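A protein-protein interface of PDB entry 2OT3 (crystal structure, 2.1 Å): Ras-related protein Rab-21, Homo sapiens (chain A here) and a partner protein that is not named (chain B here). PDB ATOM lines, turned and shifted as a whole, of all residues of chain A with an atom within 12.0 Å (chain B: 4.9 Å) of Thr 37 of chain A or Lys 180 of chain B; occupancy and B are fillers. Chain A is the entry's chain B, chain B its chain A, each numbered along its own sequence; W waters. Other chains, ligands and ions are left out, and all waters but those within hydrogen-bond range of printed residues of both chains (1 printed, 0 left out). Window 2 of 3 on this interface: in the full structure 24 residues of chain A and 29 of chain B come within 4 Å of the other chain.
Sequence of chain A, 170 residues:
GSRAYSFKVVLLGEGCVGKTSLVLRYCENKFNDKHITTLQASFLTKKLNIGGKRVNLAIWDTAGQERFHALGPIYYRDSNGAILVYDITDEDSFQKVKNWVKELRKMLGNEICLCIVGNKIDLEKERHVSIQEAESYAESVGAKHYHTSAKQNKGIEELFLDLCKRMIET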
ATOM      1  N   THR A  20      24.300 -31.736   4.949  1.00  0.00           N
ATOM      2  CA  THR A  20      23.832 -30.833   3.904  1.00  0.00           C
ATOM      3  C   THR A  20      23.607 -29.426   4.456  1.00  0.00           C
ATOM      4  O   THR A  20      23.989 -28.444   3.826  1.00  0.00           O
ATOM      5  CB  THR A  20      22.554 -31.350   3.202  1.00  0.00           C
ATOM      6  OG1 THR A  20      22.855 -32.561   2.498  1.00  0.00           O
ATOM      7  CG2 THR A  20      22.081 -30.337   2.188  1.00  0.00           C
ATOM      8  N   LEU A  24      25.505 -26.070   3.152  1.00  0.00           N
ATOM      9  CA  LEU A  24      24.667 -24.952   2.711  1.00  0.00           C
ATOM     10  C   LEU A  24      24.968 -23.697   3.539  1.00  0.00           C
ATOM     11  O   LEU A  24      25.144 -22.612   2.971  1.00  0.00           O
ATOM     12  CB  LEU A  24      23.180 -25.313   2.723  1.00  0.00           C
ATOM     13  CG  LEU A  24      22.761 -26.263   1.579  1.00  0.00           C
ATOM     14  CD1 LEU A  24      21.327 -26.734   1.752  1.00  0.00           C
ATOM     15  CD2 LEU A  24      22.973 -25.629   0.187  1.00  0.00           C
ATOM     16  N   CYS A  27      28.342 -22.468   1.983  1.00  0.00           N
ATOM     17  CA  CYS A  27      28.246 -22.014   0.600  1.00  0.00           C
ATOM     18  C   CYS A  27      26.916 -21.318   0.382  1.00  0.00           C
ATOM     19  O   CYS A  27      26.743 -20.628  -0.617  1.00  0.00           O
ATOM     20  CB  CYS A  27      28.386 -23.189  -0.367  1.00  0.00           C
ATOM     21  SG  CYS A  27      29.766 -24.279  -0.044  1.00  0.00           S
ATOM     22  N   THR A  37      15.919 -21.276  -2.827  1.00  0.00           N
ATOM     23  CA  THR A  37      16.291 -20.940  -4.217  1.00  0.00           C
ATOM     24  C   THR A  37      17.453 -21.796  -4.761  1.00  0.00           C
ATOM     25  O   THR A  37      17.573 -22.008  -5.974  1.00  0.00           O
ATOM     26  CB  THR A  37      16.623 -19.445  -4.343  1.00  0.00           C
ATOM     27  N   THR A  38      18.320 -22.257  -3.866  1.00  0.00           N
ATOM     28  CA  THR A  38      19.415 -23.153  -4.223  1.00  0.00           C
ATOM     29  C   THR A  38      18.841 -24.352  -4.981  1.00  0.00           C
ATOM     30  O   THR A  38      17.944 -25.017  -4.482  1.00  0.00           O
ATOM     31  CB  THR A  38      20.115 -23.652  -2.939  1.00  0.00           C
ATOM     32  OG1 THR A  38      20.310 -22.542  -2.058  1.00  0.00           O
ATOM     33  CG2 THR A  38      21.448 -24.313  -3.247  1.00  0.00           C
ATOM     34  N   LEU A  39      19.340 -24.606  -6.185  1.00  0.00           N
ATOM     35  CA  LEU A  39      18.876 -25.750  -6.975  1.00  0.00           C
ATOM     36  C   LEU A  39      19.279 -27.110  -6.373  1.00  0.00           C
ATOM     37  O   LEU A  39      18.469 -28.023  -6.264  1.00  0.00           O
ATOM     38  CB  LEU A  39      19.391 -25.647  -8.420  1.00  0.00           C
ATOM     39  CG  LEU A  39      19.058 -26.856  -9.331  1.00  0.00           C
ATOM     40  CD1 LEU A  39      17.550 -27.126  -9.404  1.00  0.00           C
ATOM     41  CD2 LEU A  39      19.652 -26.672 -10.726  1.00  0.00           C
ATOM     42  N   GLN A  40      20.558 -27.240  -6.023  1.00  0.00           N
ATOM     43  CA  GLN A  40      21.121 -28.527  -5.612  1.00  0.00           C
ATOM     44  C   GLN A  40      22.200 -28.330  -4.536  1.00  0.00           C
ATOM     45  O   GLN A  40      22.776 -27.227  -4.393  1.00  0.00           O
ATOM     46  CB  GLN A  40      21.662 -29.282  -6.839  1.00  0.00           C
ATOM     47  CG  GLN A  40      22.723 -28.525  -7.684  1.00  0.00           C
ATOM     48  CD  GLN A  40      24.127 -28.656  -7.122  1.00  0.00           C
ATOM     49  OE1 GLN A  40      24.406 -29.537  -6.289  1.00  0.00           O
ATOM     50  NE2 GLN A  40      25.023 -27.762  -7.554  1.00  0.00           N
ATOM     51  N   ALA A  41      22.463 -29.384  -3.769  1.00  0.00           N
ATOM     52  CA  ALA A  41      23.451 -29.305  -2.716  1.00  0.00           C
ATOM     53  C   ALA A  41      24.457 -30.444  -2.807  1.00  0.00           C
ATOM     54  O   ALA A  41      25.004 -30.867  -1.782  1.00  0.00           O
ATOM     55  CB  ALA A  41      22.756 -29.261  -1.331  1.00  0.00           C
ATOM     56  N   SER A  42      24.710 -30.930  -4.033  1.00  0.00           N
ATOM     57  CA  SER A  42      25.584 -32.079  -4.246  1.00  0.00           C
ATOM     58  C   SER A  42      26.980 -31.658  -4.679  1.00  0.00           C
ATOM     59  O   SER A  42      27.963 -32.278  -4.304  1.00  0.00           O
ATOM     60  CB  SER A  42      24.988 -33.047  -5.270  1.00  0.00           C
ATOM     61  OG  SER A  42      23.723 -33.498  -4.862  1.00  0.00           O
ATOM     62  N   PHE A  43      27.041 -30.597  -5.481  1.00  0.00           N
ATOM     63  CA  PHE A  43      28.284 -30.025  -5.925  1.00  0.00           C
ATOM     64  C   PHE A  43      28.277 -28.527  -5.613  1.00  0.00           C
ATOM     65  O   PHE A  43      27.434 -27.774  -6.102  1.00  0.00           O
ATOM     66  CB  PHE A  43      28.481 -30.229  -7.426  1.00  0.00           C
ATOM     67  CG  PHE A  43      29.732 -29.580  -7.950  1.00  0.00           C
ATOM     68  CD1 PHE A  43      30.965 -30.189  -7.768  1.00  0.00           C
ATOM     69  CD2 PHE A  43      29.683 -28.329  -8.549  1.00  0.00           C
ATOM     70  CE1 PHE A  43      32.130 -29.584  -8.233  1.00  0.00           C
ATOM     71  CE2 PHE A  43      30.840 -27.709  -9.002  1.00  0.00           C
ATOM     72  CZ  PHE A  43      32.059 -28.339  -8.860  1.00  0.00           C
ATOM     73  N   LEU A  44      29.238 -28.107  -4.811  1.00  0.00           N
ATOM     74  CA  LEU A  44      29.238 -26.770  -4.250  1.00  0.00           C
ATOM     75  C   LEU A  44      30.637 -26.209  -4.320  1.00  0.00           C
ATOM     76  O   LEU A  44      31.612 -26.939  -4.207  1.00  0.00           O
ATOM     77  CB  LEU A  44      28.727 -26.792  -2.803  1.00  0.00           C
ATOM     78  CG  LEU A  44      27.210 -27.001  -2.635  1.00  0.00           C
ATOM     79  CD1 LEU A  44      26.782 -26.981  -1.181  1.00  0.00           C
ATOM     80  CD2 LEU A  44      26.383 -25.965  -3.447  1.00  0.00           C
ATOM     81  N   PHE B 176      18.196 -32.558 -11.088  1.00  0.00           N
ATOM     82  CA  PHE B 176      18.128 -31.677  -9.936  1.00  0.00           C
ATOM     83  C   PHE B 176      16.808 -30.910  -9.873  1.00  0.00           C
ATOM     84  O   PHE B 176      16.208 -30.797  -8.804  1.00  0.00           O
ATOM     85  CB  PHE B 176      19.300 -30.693  -9.893  1.00  0.00           C
ATOM     86  CG  PHE B 176      20.614 -31.308  -9.520  1.00  0.00           C
ATOM     87  CD1 PHE B 176      20.723 -32.153  -8.425  1.00  0.00           C
ATOM     88  CD2 PHE B 176      21.765 -30.984 -10.235  1.00  0.00           C
ATOM     89  CE1 PHE B 176      21.942 -32.698  -8.070  1.00  0.00           C
ATOM     90  CE2 PHE B 176      22.995 -31.527  -9.880  1.00  0.00           C
ATOM     91  CZ  PHE B 176      23.084 -32.395  -8.808  1.00  0.00           C
ATOM     92  N   ASN B 177      16.368 -30.368 -11.011  1.00  0.00           N
ATOM     93  CA  ASN B 177      15.056 -29.716 -11.070  1.00  0.00           C
ATOM     94  C   ASN B 177      13.911 -30.661 -10.687  1.00  0.00           C
ATOM     95  O   ASN B 177      13.048 -30.293  -9.899  1.00  0.00           O
ATOM     96  CB  ASN B 177      14.810 -29.104 -12.446  1.00  0.00           C
ATOM     97  CG  ASN B 177      15.522 -27.785 -12.616  1.00  0.00           C
ATOM     98  OD1 ASN B 177      16.605 -27.694 -13.228  1.00  0.00           O
ATOM     99  ND2 ASN B 177      14.962 -26.769 -12.037  1.00  0.00           N
ATOM    100  N   ALA B 178      13.909 -31.871 -11.242  1.00  0.00           N
ATOM    101  CA  ALA B 178      12.892 -32.865 -10.892  1.00  0.00           C
ATOM    102  C   ALA B 178      12.861 -33.111  -9.368  1.00  0.00           C
ATOM    103  O   ALA B 178      11.786 -33.134  -8.750  1.00  0.00           O
ATOM    104  CB  ALA B 178      13.155 -34.172 -11.639  1.00  0.00           C
ATOM    105  N   ILE B 179      14.030 -33.270  -8.762  1.00  0.00           N
ATOM    106  CA  ILE B 179      14.096 -33.500  -7.305  1.00  0.00           C
ATOM    107  C   ILE B 179      13.650 -32.288  -6.476  1.00  0.00           C
ATOM    108  O   ILE B 179      12.909 -32.440  -5.511  1.00  0.00           O
ATOM    109  CB  ILE B 179      15.492 -33.903  -6.824  1.00  0.00           C
ATOM    110  CG1 ILE B 179      15.927 -35.253  -7.421  1.00  0.00           C
ATOM    111  CG2 ILE B 179      15.494 -33.967  -5.291  1.00  0.00           C
ATOM    112  CD1 ILE B 179      17.432 -35.546  -7.307  1.00  0.00           C
ATOM    113  N   LYS B 180      14.120 -31.095  -6.851  1.00  0.00           N
ATOM    114  CA  LYS B 180      13.757 -29.851  -6.163  1.00  0.00           C
ATOM    115  C   LYS B 180      12.249 -29.567  -6.256  1.00  0.00           C
ATOM    116  O   LYS B 180      11.648 -29.148  -5.285  1.00  0.00           O
ATOM    117  CB  LYS B 180      14.569 -28.670  -6.719  1.00  0.00           C
ATOM    118  CG  LYS B 180      14.349 -27.315  -6.029  1.00  0.00           C
ATOM    119  CD  LYS B 180      14.800 -27.338  -4.569  1.00  0.00           C
ATOM    120  CE  LYS B 180      14.500 -26.022  -3.833  1.00  0.00           C
ATOM    121  NZ  LYS B 180      15.265 -24.898  -4.432  1.00  0.00           N
ATOM    122  N   ILE B 181      11.639 -29.802  -7.415  1.00  0.00           N
ATOM    123  CA  ILE B 181      10.182 -29.602  -7.544  1.00  0.00           C
ATOM    124  C   ILE B 181       9.396 -30.577  -6.653  1.00  0.00           C
ATOM    125  O   ILE B 181       8.391 -30.196  -6.031  1.00  0.00           O
ATOM    126  CB  ILE B 181       9.679 -29.750  -9.014  1.00  0.00           C
ATOM    127  CG1 ILE B 181      10.192 -28.602  -9.895  1.00  0.00           C
ATOM    128  CG2 ILE B 181       8.140 -29.799  -9.061  1.00  0.00           C
ATOM    129  CD1 ILE B 181      10.394 -29.022 -11.390  1.00  0.00           C
ATOM    130  N   THR B 182       9.836 -31.831  -6.616  1.00  0.00           N
ATOM    131  CA  THR B 182       9.178 -32.867  -5.808  1.00  0.00           C
ATOM    132  C   THR B 182       9.326 -32.618  -4.305  1.00  0.00           C
ATOM    133  O   THR B 182       8.343 -32.728  -3.549  1.00  0.00           O
ATOM    134  CB  THR B 182       9.758 -34.260  -6.146  1.00  0.00           C
ATOM    135  OG1 THR B 182       9.511 -34.558  -7.526  1.00  0.00           O
ATOM    136  CG2 THR B 182       9.156 -35.365  -5.262  1.00  0.00           C
ATOM    137  N   LYS B 183      10.552 -32.296  -3.881  1.00  0.00           N
ATOM    138  CA  LYS B 183      10.936 -32.328  -2.466  1.00  0.00           C
ATOM    139  C   LYS B 183      10.972 -30.944  -1.842  1.00  0.00           C
ATOM    140  O   LYS B 183      10.828 -30.800  -0.625  1.00  0.00           O
ATOM    141  CB  LYS B 183      12.308 -33.005  -2.308  1.00  0.00           C
ATOM    142  CG  LYS B 183      12.286 -34.520  -2.576  1.00  0.00           C
ATOM    143  CD  LYS B 183      11.466 -35.244  -1.483  1.00  0.00           C
ATOM    144  CE  LYS B 183      11.002 -36.630  -1.909  1.00  0.00           C
ATOM    145  NZ  LYS B 183      10.426 -37.408  -0.762  1.00  0.00           N
ATOM    146  N   ASN B 184      11.186 -29.932  -2.678  1.00  0.00           N
ATOM    147  CA  ASN B 184      11.328 -28.552  -2.229  1.00  0.00           C
ATOM    148  C   ASN B 184      12.532 -28.365  -1.303  1.00  0.00           C
ATOM    149  O   ASN B 184      12.567 -27.461  -0.476  1.00  0.00           O
ATOM    150  CB  ASN B 184      10.008 -28.041  -1.620  1.00  0.00           C
ATOM    151  CG  ASN B 184       8.888 -27.966  -2.657  1.00  0.00           C
ATOM    152  OD1 ASN B 184       7.931 -28.763  -2.623  1.00  0.00           O
ATOM    153  ND2 ASN B 184       9.018 -27.028  -3.613  1.00  0.00           N
ATOM    154  N   GLU B 185      13.506 -29.261  -1.456  1.00  0.00           N
ATOM    155  CA  GLU B 185      14.820 -29.112  -0.857  1.00  0.00           C
ATOM    156  C   GLU B 185      15.851 -29.453  -1.933  1.00  0.00           C
ATOM    157  O   GLU B 185      15.566 -30.274  -2.825  1.00  0.00           O
ATOM    158  CB  GLU B 185      15.007 -30.048   0.340  1.00  0.00           C
ATOM    159  CG  GLU B 185      13.905 -30.014   1.385  1.00  0.00           C
ATOM    160  CD  GLU B 185      13.983 -28.806   2.283  1.00  0.00           C
ATOM    161  OE1 GLU B 185      14.999 -28.064   2.219  1.00  0.00           O
ATOM    162  OE2 GLU B 185      13.021 -28.604   3.060  1.00  0.00           O
ATOM    163  N   PRO B 186      17.035 -28.817  -1.863  1.00  0.00           N
ATOM    164  CA  PRO B 186      18.106 -29.085  -2.825  1.00  0.00           C
ATOM    165  C   PRO B 186      18.633 -30.510  -2.648  1.00  0.00           C
ATOM    166  O   PRO B 186      18.813 -30.964  -1.515  1.00  0.00           O
ATOM    167  CB  PRO B 186      19.188 -28.059  -2.479  1.00  0.00           C
ATOM    168  CG  PRO B 186      18.816 -27.437  -1.217  1.00  0.00           C
ATOM    169  CD  PRO B 186      17.409 -27.809  -0.849  1.00  0.00           C
HETATM  170  O   HOH W   1      17.820 -30.547  -6.359  1.00  0.00           O
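O of Thr 38 of chain A sits at hydrogen-bond distance from NZ of Lys 180 of chain B (2.7 Å).
The backbone carbonyl oxygen of Phe 43 of chain A lies within hydrogen-bond range of the side-chain amide nitrogen of Gln 40 of chain A (2.8 Å). The side-chain amide oxygen (OE1) of Gln 40 of chain A lies within hydrogen-bond range of the backbone NH (N) of Ser 42 of chain A (2.7 Å).
Among the printed residues, pairs that only touch across the chains: Leu 24 of chain A with Pro 186 of chain B, Thr 37 of chain A with Lys 180 of chain B, Thr 38 of chain A with Pro 186 of chain B, Leu 39 of chain A with Phe 176 of chain B, Leu 39 of chain A with Asn 177 of chain B, Leu 39 of chain A with Lys 180 of chain B, Leu 39 of chain A with Pro 186 of chain B, Gln 40 of chain A with Phe 176 of chain B, Gln 40 of chain A with Pro 186 of chain B, Ala 41 of chain A with Pro 186 of chain B and Ser 42 of chain A with Phe 176 of chain B.
Of the printed residues of chain B, Leu 24 of chain A touches Pro 186 (3.95 Å). Of chain B, only Lys 180 comes within 4 Å of Thr 37 of chain A. Of the printed residues of chain B, Thr 38 of chain A touches Lys 180 and Pro 186. Printed residues of chain B within 4 Å of Ser 42 of chain A: Phe 176. Leu 44 of chain A touches none of the printed residues of chain B. Of the printed residues of chain A, Phe 176 of chain B touches Leu 39 (3.9 Å), Gln 40 (3.4 Å) and Ser 42 (3.8 Å). Ala 178 of chain B touches none of the printed residues of chain A. No residue of chain A comes within 4 Å of Ile 179 of chain B. Printed residues of chain A within 4 Å of Lys 180 of chain B: Thr 37, Thr 38 and Leu 39. Ile 181 of chain B touches none of the printed residues of chain A. Thr 182 of chain B touches none of the printed residues of chain A. No residue of chain A comes within 4 Å of Asn 184 of chain B.
Of the 11 printed residues of chain B, 4 touch a printed residue of chain A. Printed residues of chain A that touch a printed residue of chain B: Leu 24, Thr 37, Thr 38, Leu 39, Gln 40, Ala 41 and Ser 42. Hydrophobic or aromatic side chains of chain A that line the printed part of chain B: Leu 24, Leu 39 and Ala 41. Among the printed residues, 12 pairs touch across the chains. Among the printed residues, no Asp or Glu carboxylate lies within 4 Å of a Lys or Arg side-chain nitrogen of the other chain.
Water W1 lies within hydrogen-bond range of O of Leu 39 of chain A (2.6 Å) and O of Phe 176 of chain B (2.9 Å).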
